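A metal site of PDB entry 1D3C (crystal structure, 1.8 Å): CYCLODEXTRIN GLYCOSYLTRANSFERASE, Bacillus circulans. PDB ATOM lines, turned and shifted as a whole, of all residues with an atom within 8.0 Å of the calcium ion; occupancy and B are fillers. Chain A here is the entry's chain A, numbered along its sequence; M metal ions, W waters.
Water W2 lies within hydrogen-bond range of O of Asn 139 (2.7 Å) and O of Leu 200 (2.8 Å).
Water W3 binds the calcium ion (2.4 Å).
The calcium ion is bound by water W1 (2.4 Å).
The calcium ion is bound by O of His 233, at 2.4 Å.
The calcium ion is bound by OD2 of Asp 199 (2.4 Å).
Water W2 binds the calcium ion, 2.5 Å away.
O of Ile 190 is bound to the calcium ion (2.5 Å).
The calcium ion is bound by OD1 of Asp 199.
The calcium ion is bound by the side-chain amide oxygen (OD1) of Asn 139, at 2.5 Å.
The calcium ion has eight donor atoms within binding distance.
The backbone carbonyl oxygen of Asn 139 lies within hydrogen-bond range of the backbone NH of Leu 200 (3.0 Å).
O of Asp 199 lies within hydrogen-bond range of N of His 176, 2.7 Å away.
The backbone NH of Asp 199 lies close to the side-chain amide oxygen of Asn 193 (3.2 Å).
The side-chain amide nitrogen (ND2) of Asn 139 is in hydrogen-bond range of a ring nitrogen (ND1) of His 140, at 3.0 Å.
N of Asn 139 is in hydrogen-bond range of SD of Met 234 (3.6 Å).
The backbone carbonyl oxygen (O) of Gly 189 sits at hydrogen-bond distance from a ring nitrogen (ND1) of His 233, 2.7 Å away.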
ATOM      1  N   PRO A 138     -20.116   1.863  12.889  1.00  0.00           N
ATOM      2  CA  PRO A 138     -20.096   1.005  11.720  1.00  0.00           C
ATOM      3  C   PRO A 138     -21.375   0.162  11.586  1.00  0.00           C
ATOM      4  O   PRO A 138     -21.446  -0.735  10.741  1.00  0.00           O
ATOM      5  CB  PRO A 138     -18.883   0.090  11.975  1.00  0.00           C
ATOM      6  CG  PRO A 138     -18.753   0.028  13.456  1.00  0.00           C
ATOM      7  CD  PRO A 138     -19.289   1.338  13.991  1.00  0.00           C
ATOM      8  N   ASN A 139     -22.376   0.449  12.396  1.00  0.00           N
ATOM      9  CA  ASN A 139     -23.626  -0.307  12.309  1.00  0.00           C
ATOM     10  C   ASN A 139     -24.406   0.029  11.066  1.00  0.00           C
ATOM     11  O   ASN A 139     -25.139  -0.810  10.542  1.00  0.00           O
ATOM     12  CB  ASN A 139     -24.524  -0.053  13.528  1.00  0.00           C
ATOM     13  CG  ASN A 139     -25.881  -0.752  13.392  1.00  0.00           C
ATOM     14  OD1 ASN A 139     -25.975  -1.982  13.437  1.00  0.00           O
ATOM     15  ND2 ASN A 139     -26.941   0.040  13.206  1.00  0.00           N
ATOM     16  N   HIS A 140     -24.309   1.273  10.615  1.00  0.00           N
ATOM     17  CA  HIS A 140     -25.098   1.723   9.502  1.00  0.00           C
ATOM     18  C   HIS A 140     -24.464   2.905   8.833  1.00  0.00           C
ATOM     19  O   HIS A 140     -23.455   3.436   9.305  1.00  0.00           O
ATOM     20  CB  HIS A 140     -26.444   2.160  10.037  1.00  0.00           C
ATOM     21  CG  HIS A 140     -26.333   3.215  11.105  1.00  0.00           C
ATOM     22  ND1 HIS A 140     -26.328   2.910  12.444  1.00  0.00           N
ATOM     23  CD2 HIS A 140     -26.098   4.536  11.026  1.00  0.00           C
ATOM     24  CE1 HIS A 140     -26.161   4.008  13.150  1.00  0.00           C
ATOM     25  NE2 HIS A 140     -26.017   5.015  12.307  1.00  0.00           N
ATOM     26  N   HIS A 176     -28.699  -4.719   4.999  1.00  0.00           N
ATOM     27  CA  HIS A 176     -29.732  -5.659   5.386  1.00  0.00           C
ATOM     28  C   HIS A 176     -31.063  -5.139   4.842  1.00  0.00           C
ATOM     29  O   HIS A 176     -31.268  -3.933   4.753  1.00  0.00           O
ATOM     30  CB  HIS A 176     -29.823  -5.767   6.923  1.00  0.00           C
ATOM     31  CG  HIS A 176     -28.796  -6.669   7.532  1.00  0.00           C
ATOM     32  ND1 HIS A 176     -28.057  -6.324   8.637  1.00  0.00           N
ATOM     33  CD2 HIS A 176     -28.378  -7.917   7.167  1.00  0.00           C
ATOM     34  CE1 HIS A 176     -27.231  -7.302   8.933  1.00  0.00           C
ATOM     35  NE2 HIS A 176     -27.401  -8.285   8.065  1.00  0.00           N
ATOM     36  N   THR A 181     -36.244  -2.856  13.234  1.00  0.00           N
ATOM     37  CA  THR A 181     -36.299  -3.520  14.535  1.00  0.00           C
ATOM     38  C   THR A 181     -37.279  -2.868  15.497  1.00  0.00           C
ATOM     39  O   THR A 181     -37.469  -1.652  15.507  1.00  0.00           O
ATOM     40  CB  THR A 181     -34.912  -3.542  15.200  1.00  0.00           C
ATOM     41  OG1 THR A 181     -35.003  -4.189  16.472  1.00  0.00           O
ATOM     42  CG2 THR A 181     -34.406  -2.122  15.392  1.00  0.00           C
ATOM     43  N   GLU A 187     -31.468 -10.501  18.579  1.00  0.00           N
ATOM     44  CA  GLU A 187     -31.294 -10.837  17.171  1.00  0.00           C
ATOM     45  C   GLU A 187     -32.109  -9.889  16.288  1.00  0.00           C
ATOM     46  O   GLU A 187     -31.686  -9.512  15.190  1.00  0.00           O
ATOM     47  CB  GLU A 187     -31.709 -12.285  16.921  1.00  0.00           C
ATOM     48  CG  GLU A 187     -32.318 -12.541  15.564  1.00  0.00           C
ATOM     49  CD  GLU A 187     -32.788 -13.979  15.401  1.00  0.00           C
ATOM     50  OE1 GLU A 187     -33.106 -14.620  16.422  1.00  0.00           O
ATOM     51  OE2 GLU A 187     -32.822 -14.459  14.236  1.00  0.00           O
ATOM     52  N   ASN A 188     -33.282  -9.488  16.784  1.00  0.00           N
ATOM     53  CA  ASN A 188     -34.145  -8.569  16.066  1.00  0.00           C
ATOM     54  C   ASN A 188     -33.455  -7.208  15.891  1.00  0.00           C
ATOM     55  O   ASN A 188     -33.484  -6.613  14.803  1.00  0.00           O
ATOM     56  CB  ASN A 188     -35.465  -8.394  16.817  1.00  0.00           C
ATOM     57  CG  ASN A 188     -36.498  -7.613  16.015  1.00  0.00           C
ATOM     58  OD1 ASN A 188     -36.324  -6.425  15.747  1.00  0.00           O
ATOM     59  ND2 ASN A 188     -37.580  -8.279  15.638  1.00  0.00           N
ATOM     60  N   GLY A 189     -32.824  -6.737  16.958  1.00  0.00           N
ATOM     61  CA  GLY A 189     -32.145  -5.439  16.929  1.00  0.00           C
ATOM     62  C   GLY A 189     -30.824  -5.475  16.146  1.00  0.00           C
ATOM     63  O   GLY A 189     -30.275  -4.443  15.822  1.00  0.00           O
ATOM     64  N   ILE A 190     -30.342  -6.667  15.848  1.00  0.00           N
ATOM     65  CA  ILE A 190     -29.082  -6.798  15.131  1.00  0.00           C
ATOM     66  C   ILE A 190     -29.228  -6.810  13.614  1.00  0.00           C
ATOM     67  O   ILE A 190     -28.575  -6.052  12.915  1.00  0.00           O
ATOM     68  CB  ILE A 190     -28.294  -8.043  15.563  1.00  0.00           C
ATOM     69  CG1 ILE A 190     -27.570  -7.789  16.887  1.00  0.00           C
ATOM     70  CG2 ILE A 190     -27.298  -8.449  14.483  1.00  0.00           C
ATOM     71  CD1 ILE A 190     -27.158  -9.058  17.593  1.00  0.00           C
ATOM     72  N   TYR A 191     -30.100  -7.681  13.109  1.00  0.00           N
ATOM     73  CA  TYR A 191     -30.256  -7.836  11.670  1.00  0.00           C
ATOM     74  C   TYR A 191     -31.384  -7.055  10.998  1.00  0.00           C
ATOM     75  O   TYR A 191     -31.712  -7.298   9.826  1.00  0.00           O
ATOM     76  CB  TYR A 191     -30.294  -9.308  11.281  1.00  0.00           C
ATOM     77  CG  TYR A 191     -29.083 -10.069  11.752  1.00  0.00           C
ATOM     78  CD1 TYR A 191     -27.913 -10.074  11.007  1.00  0.00           C
ATOM     79  CD2 TYR A 191     -29.070 -10.692  12.995  1.00  0.00           C
ATOM     80  CE1 TYR A 191     -26.789 -10.740  11.456  1.00  0.00           C
ATOM     81  CE2 TYR A 191     -27.940 -11.357  13.452  1.00  0.00           C
ATOM     82  CZ  TYR A 191     -26.800 -11.379  12.670  1.00  0.00           C
ATOM     83  OH  TYR A 191     -25.674 -12.036  13.115  1.00  0.00           O
ATOM     84  N   LYS A 192     -31.945  -6.090  11.704  1.00  0.00           N
ATOM     85  CA  LYS A 192     -32.965  -5.237  11.138  1.00  0.00           C
ATOM     86  C   LYS A 192     -32.502  -3.798  11.269  1.00  0.00           C
ATOM     87  O   LYS A 192     -31.555  -3.507  12.002  1.00  0.00           O
ATOM     88  CB  LYS A 192     -34.315  -5.470  11.790  1.00  0.00           C
ATOM     89  CG  LYS A 192     -34.993  -6.739  11.300  1.00  0.00           C
ATOM     90  CD  LYS A 192     -36.219  -7.083  12.126  1.00  0.00           C
ATOM     91  CE  LYS A 192     -36.633  -8.534  11.900  1.00  0.00           C
ATOM     92  NZ  LYS A 192     -38.107  -8.700  11.864  1.00  0.00           N
ATOM     93  N   ASN A 193     -33.102  -2.901  10.507  1.00  0.00           N
ATOM     94  CA  ASN A 193     -32.671  -1.519  10.524  1.00  0.00           C
ATOM     95  C   ASN A 193     -32.935  -0.801  11.835  1.00  0.00           C
ATOM     96  O   ASN A 193     -33.981  -0.983  12.459  1.00  0.00           O
ATOM     97  CB  ASN A 193     -33.300  -0.746   9.374  1.00  0.00           C
ATOM     98  CG  ASN A 193     -32.645  -1.036   8.049  1.00  0.00           C
ATOM     99  OD1 ASN A 193     -31.726  -1.840   7.976  1.00  0.00           O
ATOM    100  ND2 ASN A 193     -33.168  -0.444   6.989  1.00  0.00           N
ATOM    101  N   LEU A 194     -31.982   0.045  12.226  1.00  0.00           N
ATOM    102  CA  LEU A 194     -32.137   0.875  13.396  1.00  0.00           C
ATOM    103  C   LEU A 194     -32.902   2.099  12.915  1.00  0.00           C
ATOM    104  O   LEU A 194     -32.321   3.006  12.321  1.00  0.00           O
ATOM    105  CB  LEU A 194     -30.774   1.296  13.928  1.00  0.00           C
ATOM    106  CG  LEU A 194     -30.487   0.934  15.379  1.00  0.00           C
ATOM    107  CD1 LEU A 194     -29.422   1.874  15.968  1.00  0.00           C
ATOM    108  CD2 LEU A 194     -31.763   0.986  16.201  1.00  0.00           C
ATOM    109  N   LEU A 197     -32.303   3.863   9.443  1.00  0.00           N
ATOM    110  CA  LEU A 197     -30.890   3.829   9.131  1.00  0.00           C
ATOM    111  C   LEU A 197     -30.467   2.570   8.378  1.00  0.00           C
ATOM    112  O   LEU A 197     -30.748   1.460   8.805  1.00  0.00           O
ATOM    113  CB  LEU A 197     -30.065   4.022  10.397  1.00  0.00           C
ATOM    114  CG  LEU A 197     -30.340   5.321  11.160  1.00  0.00           C
ATOM    115  CD1 LEU A 197     -29.846   5.216  12.592  1.00  0.00           C
ATOM    116  CD2 LEU A 197     -29.691   6.500  10.456  1.00  0.00           C
ATOM    117  N   ALA A 198     -29.805   2.777   7.235  1.00  0.00           N
ATOM    118  CA  ALA A 198     -29.350   1.682   6.385  1.00  0.00           C
ATOM    119  C   ALA A 198     -28.443   0.739   7.151  1.00  0.00           C
ATOM    120  O   ALA A 198     -27.320   1.104   7.492  1.00  0.00           O
ATOM    121  CB  ALA A 198     -28.637   2.236   5.153  1.00  0.00           C
ATOM    122  N   ASP A 199     -28.925  -0.466   7.417  1.00  0.00           N
ATOM    123  CA  ASP A 199     -28.144  -1.426   8.190  1.00  0.00           C
ATOM    124  C   ASP A 199     -27.062  -2.109   7.374  1.00  0.00           C
ATOM    125  O   ASP A 199     -27.339  -2.841   6.427  1.00  0.00           O
ATOM    126  CB  ASP A 199     -29.046  -2.462   8.855  1.00  0.00           C
ATOM    127  CG  ASP A 199     -28.483  -2.941  10.185  1.00  0.00           C
ATOM    128  OD1 ASP A 199     -28.109  -2.083  11.023  1.00  0.00           O
ATOM    129  OD2 ASP A 199     -28.358  -4.175  10.363  1.00  0.00           O
ATOM    130  N   LEU A 200     -25.813  -1.878   7.768  1.00  0.00           N
ATOM    131  CA  LEU A 200     -24.692  -2.479   7.081  1.00  0.00           C
ATOM    132  C   LEU A 200     -24.614  -3.977   7.339  1.00  0.00           C
ATOM    133  O   LEU A 200     -24.903  -4.454   8.440  1.00  0.00           O
ATOM    134  CB  LEU A 200     -23.388  -1.793   7.482  1.00  0.00           C
ATOM    135  CG  LEU A 200     -23.170  -0.409   6.851  1.00  0.00           C
ATOM    136  CD1 LEU A 200     -21.967   0.284   7.486  1.00  0.00           C
ATOM    137  CD2 LEU A 200     -23.006  -0.523   5.338  1.00  0.00           C
ATOM    138  N   ASN A 201     -24.261  -4.733   6.298  1.00  0.00           N
ATOM    139  CA  ASN A 201     -24.169  -6.177   6.384  1.00  0.00           C
ATOM    140  C   ASN A 201     -22.711  -6.606   6.529  1.00  0.00           C
ATOM    141  O   ASN A 201     -21.963  -6.680   5.551  1.00  0.00           O
ATOM    142  CB  ASN A 201     -24.793  -6.822   5.140  1.00  0.00           C
ATOM    143  CG  ASN A 201     -24.581  -8.316   5.090  1.00  0.00           C
ATOM    144  OD1 ASN A 201     -24.181  -8.935   6.069  1.00  0.00           O
ATOM    145  ND2 ASN A 201     -24.840  -8.901   3.934  1.00  0.00           N
ATOM    146  N   HIS A 202     -22.305  -6.865   7.760  1.00  0.00           N
ATOM    147  CA  HIS A 202     -20.941  -7.241   8.060  1.00  0.00           C
ATOM    148  C   HIS A 202     -20.527  -8.616   7.551  1.00  0.00           C
ATOM    149  O   HIS A 202     -19.343  -8.941   7.568  1.00  0.00           O
ATOM    150  CB  HIS A 202     -20.653  -7.076   9.564  1.00  0.00           C
ATOM    151  CG  HIS A 202     -21.014  -5.717  10.088  1.00  0.00           C
ATOM    152  ND1 HIS A 202     -22.145  -5.480  10.840  1.00  0.00           N
ATOM    153  CD2 HIS A 202     -20.447  -4.499   9.870  1.00  0.00           C
ATOM    154  CE1 HIS A 202     -22.238  -4.191  11.101  1.00  0.00           C
ATOM    155  NE2 HIS A 202     -21.226  -3.565  10.526  1.00  0.00           N
ATOM    156  N   ALA A 230     -23.845   1.822  19.136  1.00  0.00           N
ATOM    157  CA  ALA A 230     -24.824   0.733  19.044  1.00  0.00           C
ATOM    158  C   ALA A 230     -24.256  -0.665  18.881  1.00  0.00           C
ATOM    159  O   ALA A 230     -24.601  -1.366  17.925  1.00  0.00           O
ATOM    160  CB  ALA A 230     -25.802   1.027  17.913  1.00  0.00           C
ATOM    161  N   VAL A 231     -23.421  -1.098  19.795  1.00  0.00           N
ATOM    162  CA  VAL A 231     -22.854  -2.438  19.670  1.00  0.00           C
ATOM    163  C   VAL A 231     -23.869  -3.564  19.849  1.00  0.00           C
ATOM    164  O   VAL A 231     -23.663  -4.663  19.364  1.00  0.00           O
ATOM    165  CB  VAL A 231     -21.594  -2.650  20.519  1.00  0.00           C
ATOM    166  CG1 VAL A 231     -20.609  -1.505  20.319  1.00  0.00           C
ATOM    167  CG2 VAL A 231     -21.953  -2.820  21.986  1.00  0.00           C
ATOM    168  N   LYS A 232     -24.985  -3.284  20.517  1.00  0.00           N
ATOM    169  CA  LYS A 232     -26.008  -4.302  20.690  1.00  0.00           C
ATOM    170  C   LYS A 232     -26.784  -4.480  19.373  1.00  0.00           C
ATOM    171  O   LYS A 232     -27.665  -5.329  19.282  1.00  0.00           O
ATOM    172  CB  LYS A 232     -26.964  -3.924  21.835  1.00  0.00           C
ATOM    173  CG  LYS A 232     -27.933  -2.790  21.506  1.00  0.00           C
ATOM    174  CD  LYS A 232     -28.577  -2.242  22.778  1.00  0.00           C
ATOM    175  CE  LYS A 232     -30.099  -2.225  22.684  1.00  0.00           C
ATOM    176  NZ  LYS A 232     -30.756  -2.177  24.027  1.00  0.00           N
ATOM    177  N   HIS A 233     -26.423  -3.692  18.364  1.00  0.00           N
ATOM    178  CA  HIS A 233     -27.103  -3.752  17.064  1.00  0.00           C
ATOM    179  C   HIS A 233     -26.243  -4.326  15.957  1.00  0.00           C
ATOM    180  O   HIS A 233     -26.628  -4.311  14.780  1.00  0.00           O
ATOM    181  CB  HIS A 233     -27.644  -2.391  16.692  1.00  0.00           C
ATOM    182  CG  HIS A 233     -28.736  -1.932  17.602  1.00  0.00           C
ATOM    183  ND1 HIS A 233     -29.868  -2.693  17.831  1.00  0.00           N
ATOM    184  CD2 HIS A 233     -28.801  -0.880  18.447  1.00  0.00           C
ATOM    185  CE1 HIS A 233     -30.620  -2.086  18.729  1.00  0.00           C
ATOM    186  NE2 HIS A 233     -29.996  -0.983  19.121  1.00  0.00           N
ATOM    187  N   MET A 234     -25.086  -4.854  16.326  1.00  0.00           N
ATOM    188  CA  MET A 234     -24.175  -5.470  15.367  1.00  0.00           C
ATOM    189  C   MET A 234     -23.862  -6.887  15.852  1.00  0.00           C
ATOM    190  O   MET A 234     -23.989  -7.182  17.033  1.00  0.00           O
ATOM    191  CB  MET A 234     -22.888  -4.653  15.252  1.00  0.00           C
ATOM    192  CG  MET A 234     -23.098  -3.253  14.685  1.00  0.00           C
ATOM    193  SD  MET A 234     -21.542  -2.344  14.457  1.00  0.00           S
ATOM    194  CE  MET A 234     -21.470  -1.398  15.977  1.00  0.00           C
ATOM    195  N   PRO A 235     -23.471  -7.767  14.937  1.00  0.00           N
ATOM    196  CA  PRO A 235     -23.165  -9.135  15.316  1.00  0.00           C
ATOM    197  C   PRO A 235     -21.982  -9.139  16.284  1.00  0.00           C
ATOM    198  O   PRO A 235     -20.954  -8.506  16.033  1.00  0.00           O
ATOM    199  CB  PRO A 235     -22.761  -9.774  13.999  1.00  0.00           C
ATOM    200  CG  PRO A 235     -23.476  -9.004  12.973  1.00  0.00           C
ATOM    201  CD  PRO A 235     -23.513  -7.599  13.468  1.00  0.00           C
HETATM  202 CA    CA M   1     -27.255  -3.947  12.497  1.00  0.00          CA
HETATM  203  O   HOH W   1     -29.246  -3.107  13.513  1.00  0.00           O
HETATM  204  O   HOH W   2     -25.325  -3.445  11.071  1.00  0.00           O
HETATM  205  O   HOH W   3     -25.955  -5.918  12.267  1.00  0.00           O
